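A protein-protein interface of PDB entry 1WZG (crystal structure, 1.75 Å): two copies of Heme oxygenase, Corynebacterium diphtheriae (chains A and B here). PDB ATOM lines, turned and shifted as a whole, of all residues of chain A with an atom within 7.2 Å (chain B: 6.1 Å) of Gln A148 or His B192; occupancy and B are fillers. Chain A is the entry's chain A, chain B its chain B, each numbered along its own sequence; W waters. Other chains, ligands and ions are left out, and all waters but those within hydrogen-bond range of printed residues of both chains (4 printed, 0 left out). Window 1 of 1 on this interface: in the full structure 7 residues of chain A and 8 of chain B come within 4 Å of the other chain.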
ATOM      1  N   VAL A 142     -21.153 -18.670 -33.217  1.00  0.00           N
ATOM      2  CA  VAL A 142     -21.747 -19.705 -32.380  1.00  0.00           C
ATOM      3  C   VAL A 142     -21.162 -21.065 -32.773  1.00  0.00           C
ATOM      4  O   VAL A 142     -20.618 -21.790 -31.905  1.00  0.00           O
ATOM      5  CB  VAL A 142     -23.308 -19.689 -32.447  1.00  0.00           C
ATOM      6  CG1 VAL A 142     -23.909 -20.960 -31.818  1.00  0.00           C
ATOM      7  CG2 VAL A 142     -23.826 -18.415 -31.779  1.00  0.00           C
ATOM      8  N   ILE A 143     -21.232 -21.383 -34.064  1.00  0.00           N
ATOM      9  CA  ILE A 143     -20.720 -22.672 -34.552  1.00  0.00           C
ATOM     10  C   ILE A 143     -19.219 -22.761 -34.297  1.00  0.00           C
ATOM     11  O   ILE A 143     -18.745 -23.780 -33.814  1.00  0.00           O
ATOM     12  CB  ILE A 143     -21.015 -22.921 -36.043  1.00  0.00           C
ATOM     13  CG1 ILE A 143     -22.532 -22.932 -36.303  1.00  0.00           C
ATOM     14  CG2 ILE A 143     -20.417 -24.250 -36.486  1.00  0.00           C
ATOM     15  CD1 ILE A 143     -22.884 -23.298 -37.762  1.00  0.00           C
ATOM     16  N   ALA A 144     -18.479 -21.699 -34.588  1.00  0.00           N
ATOM     17  CA  ALA A 144     -17.036 -21.686 -34.291  1.00  0.00           C
ATOM     18  C   ALA A 144     -16.723 -21.967 -32.806  1.00  0.00           C
ATOM     19  O   ALA A 144     -15.823 -22.754 -32.479  1.00  0.00           O
ATOM     20  CB  ALA A 144     -16.441 -20.336 -34.709  1.00  0.00           C
ATOM     21  N   ARG A 145     -17.448 -21.291 -31.915  1.00  0.00           N
ATOM     22  CA  ARG A 145     -17.251 -21.468 -30.473  1.00  0.00           C
ATOM     23  C   ARG A 145     -17.541 -22.913 -30.115  1.00  0.00           C
ATOM     24  O   ARG A 145     -16.818 -23.514 -29.312  1.00  0.00           O
ATOM     25  CB  ARG A 145     -18.124 -20.521 -29.641  1.00  0.00           C
ATOM     26  CG  ARG A 145     -18.003 -20.680 -28.081  1.00  0.00           C
ATOM     27  CD  ARG A 145     -16.541 -20.633 -27.562  1.00  0.00           C
ATOM     28  NE  ARG A 145     -16.413 -20.258 -26.139  1.00  0.00           N
ATOM     29  CZ  ARG A 145     -16.220 -18.998 -25.715  1.00  0.00           C
ATOM     30  NH1 ARG A 145     -16.090 -18.005 -26.587  1.00  0.00           N
ATOM     31  NH2 ARG A 145     -16.129 -18.732 -24.413  1.00  0.00           N
ATOM     32  N   MET A 146     -18.586 -23.465 -30.713  1.00  0.00           N
ATOM     33  CA  MET A 146     -18.939 -24.864 -30.448  1.00  0.00           C
ATOM     34  C   MET A 146     -17.871 -25.858 -30.913  1.00  0.00           C
ATOM     35  O   MET A 146     -17.629 -26.873 -30.251  1.00  0.00           O
ATOM     36  CB  MET A 146     -20.327 -25.228 -31.023  1.00  0.00           C
ATOM     37  CG  MET A 146     -21.505 -24.519 -30.326  1.00  0.00           C
ATOM     38  SD  MET A 146     -21.567 -24.847 -28.541  1.00  0.00           S
ATOM     39  CE  MET A 146     -20.430 -23.686 -27.924  1.00  0.00           C
ATOM     40  N   MET A 147     -17.245 -25.574 -32.054  1.00  0.00           N
ATOM     41  CA  MET A 147     -16.230 -26.488 -32.571  1.00  0.00           C
ATOM     42  C   MET A 147     -14.981 -26.464 -31.684  1.00  0.00           C
ATOM     43  O   MET A 147     -14.302 -27.463 -31.535  1.00  0.00           O
ATOM     44  CB  MET A 147     -15.871 -26.156 -34.013  1.00  0.00           C
ATOM     45  CG  MET A 147     -17.062 -26.289 -35.046  1.00  0.00           C
ATOM     46  SD  MET A 147     -17.951 -27.844 -34.984  1.00  0.00           S
ATOM     47  CE  MET A 147     -19.194 -27.474 -33.753  1.00  0.00           C
ATOM     48  N   GLN A 148     -14.680 -25.324 -31.094  1.00  0.00           N
ATOM     49  CA  GLN A 148     -13.571 -25.260 -30.134  1.00  0.00           C
ATOM     50  C   GLN A 148     -13.969 -25.973 -28.838  1.00  0.00           C
ATOM     51  O   GLN A 148     -13.210 -26.807 -28.318  1.00  0.00           O
ATOM     52  CB  GLN A 148     -13.167 -23.827 -29.819  1.00  0.00           C
ATOM     53  CG  GLN A 148     -12.565 -23.061 -31.008  1.00  0.00           C
ATOM     54  CD  GLN A 148     -11.782 -21.872 -30.551  1.00  0.00           C
ATOM     55  OE1 GLN A 148     -12.165 -20.734 -30.820  1.00  0.00           O
ATOM     56  NE2 GLN A 148     -10.676 -22.123 -29.839  1.00  0.00           N
ATOM     57  N   ARG A 149     -15.186 -25.707 -28.355  1.00  0.00           N
ATOM     58  CA  ARG A 149     -15.620 -26.215 -27.048  1.00  0.00           C
ATOM     59  C   ARG A 149     -15.760 -27.722 -27.056  1.00  0.00           C
ATOM     60  O   ARG A 149     -15.342 -28.382 -26.131  1.00  0.00           O
ATOM     61  CB  ARG A 149     -16.937 -25.560 -26.605  1.00  0.00           C
ATOM     62  CG  ARG A 149     -17.568 -26.243 -25.361  1.00  0.00           C
ATOM     63  CD  ARG A 149     -18.832 -25.491 -24.832  1.00  0.00           C
ATOM     64  NE  ARG A 149     -18.608 -24.057 -24.671  1.00  0.00           N
ATOM     65  CZ  ARG A 149     -19.570 -23.151 -24.445  1.00  0.00           C
ATOM     66  NH1 ARG A 149     -20.831 -23.527 -24.340  1.00  0.00           N
ATOM     67  NH2 ARG A 149     -19.262 -21.871 -24.336  1.00  0.00           N
ATOM     68  N   HIS A 150     -16.352 -28.257 -28.121  1.00  0.00           N
ATOM     69  CA  HIS A 150     -16.673 -29.671 -28.164  1.00  0.00           C
ATOM     70  C   HIS A 150     -15.584 -30.502 -28.775  1.00  0.00           C
ATOM     71  O   HIS A 150     -15.382 -31.624 -28.339  1.00  0.00           O
ATOM     72  CB  HIS A 150     -17.983 -29.922 -28.918  1.00  0.00           C
ATOM     73  CG  HIS A 150     -19.194 -29.464 -28.166  1.00  0.00           C
ATOM     74  ND1 HIS A 150     -19.347 -29.676 -26.809  1.00  0.00           N
ATOM     75  CD2 HIS A 150     -20.316 -28.830 -28.577  1.00  0.00           C
ATOM     76  CE1 HIS A 150     -20.496 -29.156 -26.413  1.00  0.00           C
ATOM     77  NE2 HIS A 150     -21.108 -28.651 -27.468  1.00  0.00           N
ATOM     78  N   TYR A 151     -14.863 -29.956 -29.759  1.00  0.00           N
ATOM     79  CA  TYR A 151     -13.957 -30.794 -30.568  1.00  0.00           C
ATOM     80  C   TYR A 151     -12.522 -30.311 -30.592  1.00  0.00           C
ATOM     81  O   TYR A 151     -11.689 -30.888 -31.298  1.00  0.00           O
ATOM     82  CB  TYR A 151     -14.504 -30.969 -31.994  1.00  0.00           C
ATOM     83  CG  TYR A 151     -15.958 -31.400 -31.993  1.00  0.00           C
ATOM     84  CD1 TYR A 151     -16.937 -30.614 -32.593  1.00  0.00           C
ATOM     85  CD2 TYR A 151     -16.351 -32.570 -31.339  1.00  0.00           C
ATOM     86  CE1 TYR A 151     -18.275 -30.993 -32.585  1.00  0.00           C
ATOM     87  CE2 TYR A 151     -17.693 -32.956 -31.320  1.00  0.00           C
ATOM     88  CZ  TYR A 151     -18.643 -32.172 -31.933  1.00  0.00           C
ATOM     89  OH  TYR A 151     -19.950 -32.583 -31.891  1.00  0.00           O
ATOM     90  N   GLY A 152     -12.234 -29.263 -29.823  1.00  0.00           N
ATOM     91  CA  GLY A 152     -10.887 -28.734 -29.679  1.00  0.00           C
ATOM     92  C   GLY A 152     -10.293 -28.243 -30.981  1.00  0.00           C
ATOM     93  O   GLY A 152      -9.075 -28.287 -31.157  1.00  0.00           O
ATOM     94  N   VAL A 153     -11.143 -27.782 -31.904  1.00  0.00           N
ATOM     95  CA  VAL A 153     -10.630 -27.314 -33.207  1.00  0.00           C
ATOM     96  C   VAL A 153      -9.755 -26.079 -33.040  1.00  0.00           C
ATOM     97  O   VAL A 153     -10.127 -25.125 -32.360  1.00  0.00           O
ATOM     98  CB  VAL A 153     -11.773 -27.038 -34.233  1.00  0.00           C
ATOM     99  CG1 VAL A 153     -11.238 -26.504 -35.570  1.00  0.00           C
ATOM    100  CG2 VAL A 153     -12.541 -28.301 -34.501  1.00  0.00           C
ATOM    101  N   ASP A 154      -8.579 -26.117 -33.665  1.00  0.00           N
ATOM    102  CA  ASP A 154      -7.669 -24.953 -33.664  1.00  0.00           C
ATOM    103  C   ASP A 154      -8.388 -23.726 -34.250  1.00  0.00           C
ATOM    104  O   ASP A 154      -8.901 -23.796 -35.365  1.00  0.00           O
ATOM    105  CB  ASP A 154      -6.443 -25.344 -34.482  1.00  0.00           C
ATOM    106  CG  ASP A 154      -5.414 -24.225 -34.651  1.00  0.00           C
ATOM    107  OD1 ASP A 154      -5.564 -23.086 -34.131  1.00  0.00           O
ATOM    108  OD2 ASP A 154      -4.402 -24.535 -35.341  1.00  0.00           O
ATOM    109  N   PRO A 155      -8.413 -22.589 -33.509  1.00  0.00           N
ATOM    110  CA  PRO A 155      -9.093 -21.411 -34.060  1.00  0.00           C
ATOM    111  C   PRO A 155      -8.516 -21.015 -35.412  1.00  0.00           C
ATOM    112  O   PRO A 155      -9.191 -20.399 -36.201  1.00  0.00           O
ATOM    113  CB  PRO A 155      -8.854 -20.307 -33.011  1.00  0.00           C
ATOM    114  CG  PRO A 155      -7.891 -20.841 -32.065  1.00  0.00           C
ATOM    115  CD  PRO A 155      -7.846 -22.336 -32.176  1.00  0.00           C
ATOM    116  N   GLU A 156      -7.264 -21.380 -35.678  1.00  0.00           N
ATOM    117  CA  GLU A 156      -6.678 -21.090 -36.990  1.00  0.00           C
ATOM    118  C   GLU A 156      -7.277 -21.906 -38.127  1.00  0.00           C
ATOM    119  O   GLU A 156      -7.089 -21.554 -39.301  1.00  0.00           O
ATOM    120  CB  GLU A 156      -5.183 -21.308 -36.973  1.00  0.00           C
ATOM    121  CG  GLU A 156      -4.446 -20.183 -36.350  1.00  0.00           C
ATOM    122  CD  GLU A 156      -3.138 -19.965 -37.066  1.00  0.00           C
ATOM    123  OE1 GLU A 156      -2.201 -20.732 -36.797  1.00  0.00           O
ATOM    124  OE2 GLU A 156      -3.059 -19.049 -37.920  1.00  0.00           O
ATOM    125  N   LEU A 158     -10.508 -22.334 -38.239  1.00  0.00           N
ATOM    126  CA  LEU A 158     -11.890 -21.858 -38.297  1.00  0.00           C
ATOM    127  C   LEU A 158     -11.945 -20.527 -39.039  1.00  0.00           C
ATOM    128  O   LEU A 158     -12.814 -19.671 -38.767  1.00  0.00           O
ATOM    129  CB  LEU A 158     -12.466 -21.725 -36.880  1.00  0.00           C
ATOM    130  CG  LEU A 158     -12.542 -23.007 -36.045  1.00  0.00           C
ATOM    131  CD1 LEU A 158     -12.893 -22.707 -34.591  1.00  0.00           C
ATOM    132  CD2 LEU A 158     -13.603 -23.933 -36.686  1.00  0.00           C
ATOM    133  N   ASP B 121      -4.858 -32.883 -29.360  1.00  0.00           N
ATOM    134  CA  ASP B 121      -5.767 -32.016 -28.604  1.00  0.00           C
ATOM    135  C   ASP B 121      -5.364 -31.974 -27.149  1.00  0.00           C
ATOM    136  O   ASP B 121      -5.733 -32.871 -26.340  1.00  0.00           O
ATOM    137  CB  ASP B 121      -7.179 -32.551 -28.774  1.00  0.00           C
ATOM    138  CG  ASP B 121      -8.233 -31.665 -28.138  1.00  0.00           C
ATOM    139  OD1 ASP B 121      -7.903 -30.734 -27.376  1.00  0.00           O
ATOM    140  OD2 ASP B 121      -9.413 -31.947 -28.421  1.00  0.00           O
ATOM    141  N   PRO B 123      -5.818 -29.837 -24.407  1.00  0.00           N
ATOM    142  CA  PRO B 123      -6.851 -29.721 -23.376  1.00  0.00           C
ATOM    143  C   PRO B 123      -7.653 -31.027 -23.184  1.00  0.00           C
ATOM    144  O   PRO B 123      -7.825 -31.494 -22.049  1.00  0.00           O
ATOM    145  CB  PRO B 123      -7.741 -28.589 -23.907  1.00  0.00           C
ATOM    146  CG  PRO B 123      -6.752 -27.685 -24.634  1.00  0.00           C
ATOM    147  CD  PRO B 123      -5.901 -28.721 -25.376  1.00  0.00           C
ATOM    148  N   ALA B 124      -8.100 -31.622 -24.277  1.00  0.00           N
ATOM    149  CA  ALA B 124      -8.792 -32.906 -24.181  1.00  0.00           C
ATOM    150  C   ALA B 124      -7.952 -33.996 -23.495  1.00  0.00           C
ATOM    151  O   ALA B 124      -8.447 -34.760 -22.624  1.00  0.00           O
ATOM    152  CB  ALA B 124      -9.261 -33.356 -25.526  1.00  0.00           C
ATOM    153  N   ALA B 127      -7.765 -33.595 -19.765  1.00  0.00           N
ATOM    154  CA  ALA B 127      -9.016 -34.087 -19.166  1.00  0.00           C
ATOM    155  C   ALA B 127      -8.993 -35.608 -18.935  1.00  0.00           C
ATOM    156  O   ALA B 127      -9.282 -36.075 -17.836  1.00  0.00           O
ATOM    157  CB  ALA B 127     -10.217 -33.697 -19.995  1.00  0.00           C
ATOM    158  N   SER B 186      -6.963 -20.862 -23.065  1.00  0.00           N
ATOM    159  CA  SER B 186      -7.981 -19.884 -23.498  1.00  0.00           C
ATOM    160  C   SER B 186      -9.314 -20.291 -22.860  1.00  0.00           C
ATOM    161  O   SER B 186      -9.433 -21.420 -22.345  1.00  0.00           O
ATOM    162  CB  SER B 186      -8.134 -19.878 -25.010  1.00  0.00           C
ATOM    163  OG  SER B 186      -8.681 -21.123 -25.420  1.00  0.00           O
ATOM    164  N   ASP B 187     -10.305 -19.399 -22.870  1.00  0.00           N
ATOM    165  CA  ASP B 187     -11.638 -19.757 -22.344  1.00  0.00           C
ATOM    166  C   ASP B 187     -12.167 -20.989 -23.071  1.00  0.00           C
ATOM    167  O   ASP B 187     -12.779 -21.872 -22.488  1.00  0.00           O
ATOM    168  CB  ASP B 187     -12.659 -18.620 -22.529  1.00  0.00           C
ATOM    169  CG  ASP B 187     -12.332 -17.366 -21.707  1.00  0.00           C
ATOM    170  OD1 ASP B 187     -11.469 -17.409 -20.792  1.00  0.00           O
ATOM    171  OD2 ASP B 187     -12.977 -16.337 -21.998  1.00  0.00           O
ATOM    172  N   GLU B 188     -11.942 -21.032 -24.375  1.00  0.00           N
ATOM    173  CA  GLU B 188     -12.442 -22.135 -25.186  1.00  0.00           C
ATOM    174  C   GLU B 188     -11.741 -23.443 -24.843  1.00  0.00           C
ATOM    175  O   GLU B 188     -12.400 -24.483 -24.714  1.00  0.00           O
ATOM    176  CB  GLU B 188     -12.305 -21.807 -26.673  1.00  0.00           C
ATOM    177  CG  GLU B 188     -13.120 -20.573 -27.088  1.00  0.00           C
ATOM    178  CD  GLU B 188     -12.305 -19.286 -27.113  1.00  0.00           C
ATOM    179  OE1 GLU B 188     -12.689 -18.373 -27.864  1.00  0.00           O
ATOM    180  OE2 GLU B 188     -11.290 -19.158 -26.406  1.00  0.00           O
ATOM    181  N   GLN B 189     -10.420 -23.396 -24.680  1.00  0.00           N
ATOM    182  CA  GLN B 189      -9.676 -24.595 -24.256  1.00  0.00           C
ATOM    183  C   GLN B 189     -10.147 -25.077 -22.890  1.00  0.00           C
ATOM    184  O   GLN B 189     -10.243 -26.284 -22.650  1.00  0.00           O
ATOM    185  CB  GLN B 189      -8.182 -24.325 -24.191  1.00  0.00           C
ATOM    186  CG  GLN B 189      -7.538 -24.142 -25.549  1.00  0.00           C
ATOM    187  CD  GLN B 189      -6.089 -23.753 -25.450  1.00  0.00           C
ATOM    188  OE1 GLN B 189      -5.744 -22.824 -24.730  1.00  0.00           O
ATOM    189  NE2 GLN B 189      -5.225 -24.460 -26.185  1.00  0.00           N
ATOM    190  N   ARG B 190     -10.440 -24.126 -21.996  1.00  0.00           N
ATOM    191  CA  ARG B 190     -10.851 -24.483 -20.636  1.00  0.00           C
ATOM    192  C   ARG B 190     -12.207 -25.183 -20.688  1.00  0.00           C
ATOM    193  O   ARG B 190     -12.402 -26.260 -20.082  1.00  0.00           O
ATOM    194  CB  ARG B 190     -10.879 -23.249 -19.716  1.00  0.00           C
ATOM    195  CG  ARG B 190     -11.070 -23.602 -18.222  1.00  0.00           C
ATOM    196  CD  ARG B 190     -10.863 -22.387 -17.287  1.00  0.00           C
ATOM    197  NE  ARG B 190     -11.462 -22.634 -15.967  1.00  0.00           N
ATOM    198  CZ  ARG B 190     -10.957 -22.215 -14.799  1.00  0.00           C
ATOM    199  NH1 ARG B 190      -9.826 -21.514 -14.755  1.00  0.00           N
ATOM    200  NH2 ARG B 190     -11.580 -22.507 -13.658  1.00  0.00           N
ATOM    201  N   GLU B 191     -13.146 -24.582 -21.418  1.00  0.00           N
ATOM    202  CA  GLU B 191     -14.440 -25.190 -21.659  1.00  0.00           C
ATOM    203  C   GLU B 191     -14.325 -26.581 -22.238  1.00  0.00           C
ATOM    204  O   GLU B 191     -15.077 -27.477 -21.833  1.00  0.00           O
ATOM    205  CB  GLU B 191     -15.279 -24.314 -22.605  1.00  0.00           C
ATOM    206  CG  GLU B 191     -15.749 -23.022 -21.920  1.00  0.00           C
ATOM    207  CD  GLU B 191     -16.340 -22.019 -22.915  1.00  0.00           C
ATOM    208  OE1 GLU B 191     -16.625 -22.438 -24.061  1.00  0.00           O
ATOM    209  OE2 GLU B 191     -16.527 -20.822 -22.552  1.00  0.00           O
ATOM    210  N   HIS B 192     -13.384 -26.755 -23.180  1.00  0.00           N
ATOM    211  CA  HIS B 192     -13.178 -28.061 -23.864  1.00  0.00           C
ATOM    212  C   HIS B 192     -12.647 -29.121 -22.897  1.00  0.00           C
ATOM    213  O   HIS B 192     -13.145 -30.263 -22.838  1.00  0.00           O
ATOM    214  CB  HIS B 192     -12.246 -27.886 -25.084  1.00  0.00           C
ATOM    215  CG  HIS B 192     -12.026 -29.143 -25.885  1.00  0.00           C
ATOM    216  ND1 HIS B 192     -13.062 -29.939 -26.316  1.00  0.00           N
ATOM    217  CD2 HIS B 192     -10.894 -29.723 -26.352  1.00  0.00           C
ATOM    218  CE1 HIS B 192     -12.587 -30.967 -26.996  1.00  0.00           C
ATOM    219  NE2 HIS B 192     -11.273 -30.858 -27.037  1.00  0.00           N
ATOM    220  N   LEU B 193     -11.685 -28.709 -22.093  1.00  0.00           N
ATOM    221  CA  LEU B 193     -11.128 -29.581 -21.065  1.00  0.00           C
ATOM    222  C   LEU B 193     -12.224 -30.055 -20.103  1.00  0.00           C
ATOM    223  O   LEU B 193     -12.321 -31.249 -19.793  1.00  0.00           O
ATOM    224  CB  LEU B 193     -10.004 -28.843 -20.310  1.00  0.00           C
ATOM    225  CG  LEU B 193      -9.117 -29.664 -19.374  1.00  0.00           C
ATOM    226  CD1 LEU B 193      -7.793 -28.908 -19.137  1.00  0.00           C
ATOM    227  CD2 LEU B 193      -9.833 -29.900 -18.014  1.00  0.00           C
ATOM    228  N   LEU B 194     -13.078 -29.123 -19.668  1.00  0.00           N
ATOM    229  CA  LEU B 194     -14.166 -29.470 -18.740  1.00  0.00           C
ATOM    230  C   LEU B 194     -15.171 -30.430 -19.381  1.00  0.00           C
ATOM    231  O   LEU B 194     -15.570 -31.420 -18.761  1.00  0.00           O
ATOM    232  CB  LEU B 194     -14.864 -28.217 -18.213  1.00  0.00           C
ATOM    233  CG  LEU B 194     -14.003 -27.303 -17.332  1.00  0.00           C
ATOM    234  CD1 LEU B 194     -14.717 -25.963 -17.039  1.00  0.00           C
ATOM    235  CD2 LEU B 194     -13.574 -28.018 -16.039  1.00  0.00           C
ATOM    236  N   LYS B 195     -15.506 -30.175 -20.642  1.00  0.00           N
ATOM    237  CA  LYS B 195     -16.445 -31.019 -21.406  1.00  0.00           C
ATOM    238  C   LYS B 195     -15.888 -32.440 -21.564  1.00  0.00           C
ATOM    239  O   LYS B 195     -16.586 -33.435 -21.278  1.00  0.00           O
ATOM    240  CB  LYS B 195     -16.778 -30.317 -22.744  1.00  0.00           C
ATOM    241  CG  LYS B 195     -16.717 -31.068 -24.125  1.00  0.00           C
ATOM    242  CD  LYS B 195     -17.624 -32.304 -24.327  1.00  0.00           C
ATOM    243  CE  LYS B 195     -18.074 -32.492 -25.804  1.00  0.00           C
ATOM    244  NZ  LYS B 195     -18.043 -33.921 -26.351  1.00  0.00           N
ATOM    245  N   GLU B 196     -14.628 -32.520 -21.983  1.00  0.00           N
ATOM    246  CA  GLU B 196     -13.964 -33.828 -22.152  1.00  0.00           C
ATOM    247  C   GLU B 196     -13.875 -34.595 -20.841  1.00  0.00           C
ATOM    248  O   GLU B 196     -13.967 -35.831 -20.851  1.00  0.00           O
ATOM    249  CB  GLU B 196     -12.582 -33.693 -22.820  1.00  0.00           C
ATOM    250  CG  GLU B 196     -12.708 -33.377 -24.355  1.00  0.00           C
ATOM    251  CD  GLU B 196     -13.010 -34.620 -25.230  1.00  0.00           C
ATOM    252  OE1 GLU B 196     -13.306 -34.411 -26.416  1.00  0.00           O
ATOM    253  OE2 GLU B 196     -12.904 -35.789 -24.770  1.00  0.00           O
ATOM    254  N   ALA B 197     -13.685 -33.887 -19.724  1.00  0.00           N
ATOM    255  CA  ALA B 197     -13.549 -34.577 -18.420  1.00  0.00           C
ATOM    256  C   ALA B 197     -14.834 -35.296 -18.029  1.00  0.00           C
ATOM    257  O   ALA B 197     -14.796 -36.452 -17.572  1.00  0.00           O
ATOM    258  CB  ALA B 197     -13.081 -33.629 -17.331  1.00  0.00           C
HETATM  259  O   HOH W   1     -10.666 -18.346 -30.157  1.00  0.00           O
HETATM  260  O   HOH W   2      -8.663 -20.885 -28.079  1.00  0.00           O
HETATM  261  O   HOH W   3     -15.527 -16.249 -23.249  1.00  0.00           O
HETATM  262  O   HOH W   4     -15.450 -34.236 -27.837  1.00  0.00           O
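OE1 of Glu B188 is in salt-bridge range of NH1 of Arg A145, at 3.7 Å.
The guanidinium group (NH2) of Arg A145 lies within salt-bridge range of the side-chain carboxylate (OE2) of Glu B191.
The guanidinium group (NE) of Arg A149 is in salt-bridge range of the side-chain carboxylate (OE1) of Glu B191.
O of Arg A149 is in hydrogen-bond range of ND1 of His B192 (2.8 Å).
The backbone NH (N) of Gly A152 sits close to a ring nitrogen (NE2) of His B192, 3.4 Å away.
The backbone NH of Gly A152 lies within hydrogen-bond range of the backbone carbonyl oxygen of Met A147.
OD1 of Asp B121 lies within hydrogen-bond range of N of Ala B124 (3.2 Å).
A ring nitrogen (NE2) of His B192 is in hydrogen-bond range of the side-chain carboxylate (OD2) of Asp B121 (2.6 Å).
OE2 of Glu B188 lies within hydrogen-bond range of OG of Ser B186.
Among the printed residues, merely in contact across the chains: Arg A145 with Asp B187 (3.95 Å), Gln A148 with Glu B188 (3.6 Å), Gln A148 with His B192 (3.5 Å), Arg A149 with Lys B195 (3.6 Å), His A150 with His B192 (3.2 Å), His A150 with Lys B195 (3.2 Å), His A150 with Glu B196 (3.97 Å), Tyr A151 with Asp B121 (3.8 Å), Tyr A151 with His B192 (3.7 Å) and Gly A152 with Asp B121 (3.8 Å).
Of chain B, only Glu B188 and His B192 come within 4 Å of Gln A148.
His B192 touches five residues of chain A.
Of the printed residues of chain B, Arg A149 touches Glu B191, His B192 and Lys B195.
Printed residues of chain B within 4 Å of Gly A152: Asp B121 (3.8 Å) and His B192 (3.3 Å).
Pro A155 touches none of the printed residues of chain B.
Ile A143 touches none of the printed residues of chain B.
The nearest residue of chain A that does not touch His B192 is Val A153 (5.8 Å).
The nearest printed residue of chain A that does not touch Glu B188 is Arg A149 (4.3 Å).
Hydrophobic or aromatic side chains of chain A within 4 Å of the printed part of chain B: His A150.
Printed residues of chain B that touch a printed residue of chain A: Asp B121, Asp B187, Glu B188, Glu B191, His B192, Lys B195 and Glu B196.
Hydrophobic or aromatic side chains of chain B that line the printed part of chain A: His B192.
Among the printed residues, 15 pairs touch across the chains.
Among the printed residues, Asp or Glu carboxylates within 4 Å of a Lys or Arg side-chain nitrogen of the other chain: Arg A145 with Glu B188 (3.7 Å), Arg A145 with Glu B191 (2.8 Å) and Arg A149 with Glu B191 (2.6 Å).
No position is printed for both chains.
Of the 15 pairs that touch across the chains among the printed residues, none has its exchanged pair printed and touching as well.
Water W4 lies within hydrogen-bond range of OE1 of Glu B196 (2.6 Å), O of His A150 (2.7 Å) and NZ of Lys B195 (3.0 Å).
Water W2 lies within hydrogen-bond range of the side-chain hydroxyl (OG) of Ser B186 (2.7 Å) and the side-chain amide nitrogen (NE2) of Gln A148 (2.9 Å).
Water W3 bridges the guanidinium group of Arg A145 (2.8 Å) and the side-chain carboxylate of Asp B187 (2.8 Å).
Water W1 bridges OE1 of Gln A148 (2.9 Å) and OE1 of Glu B188 (3.1 Å).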
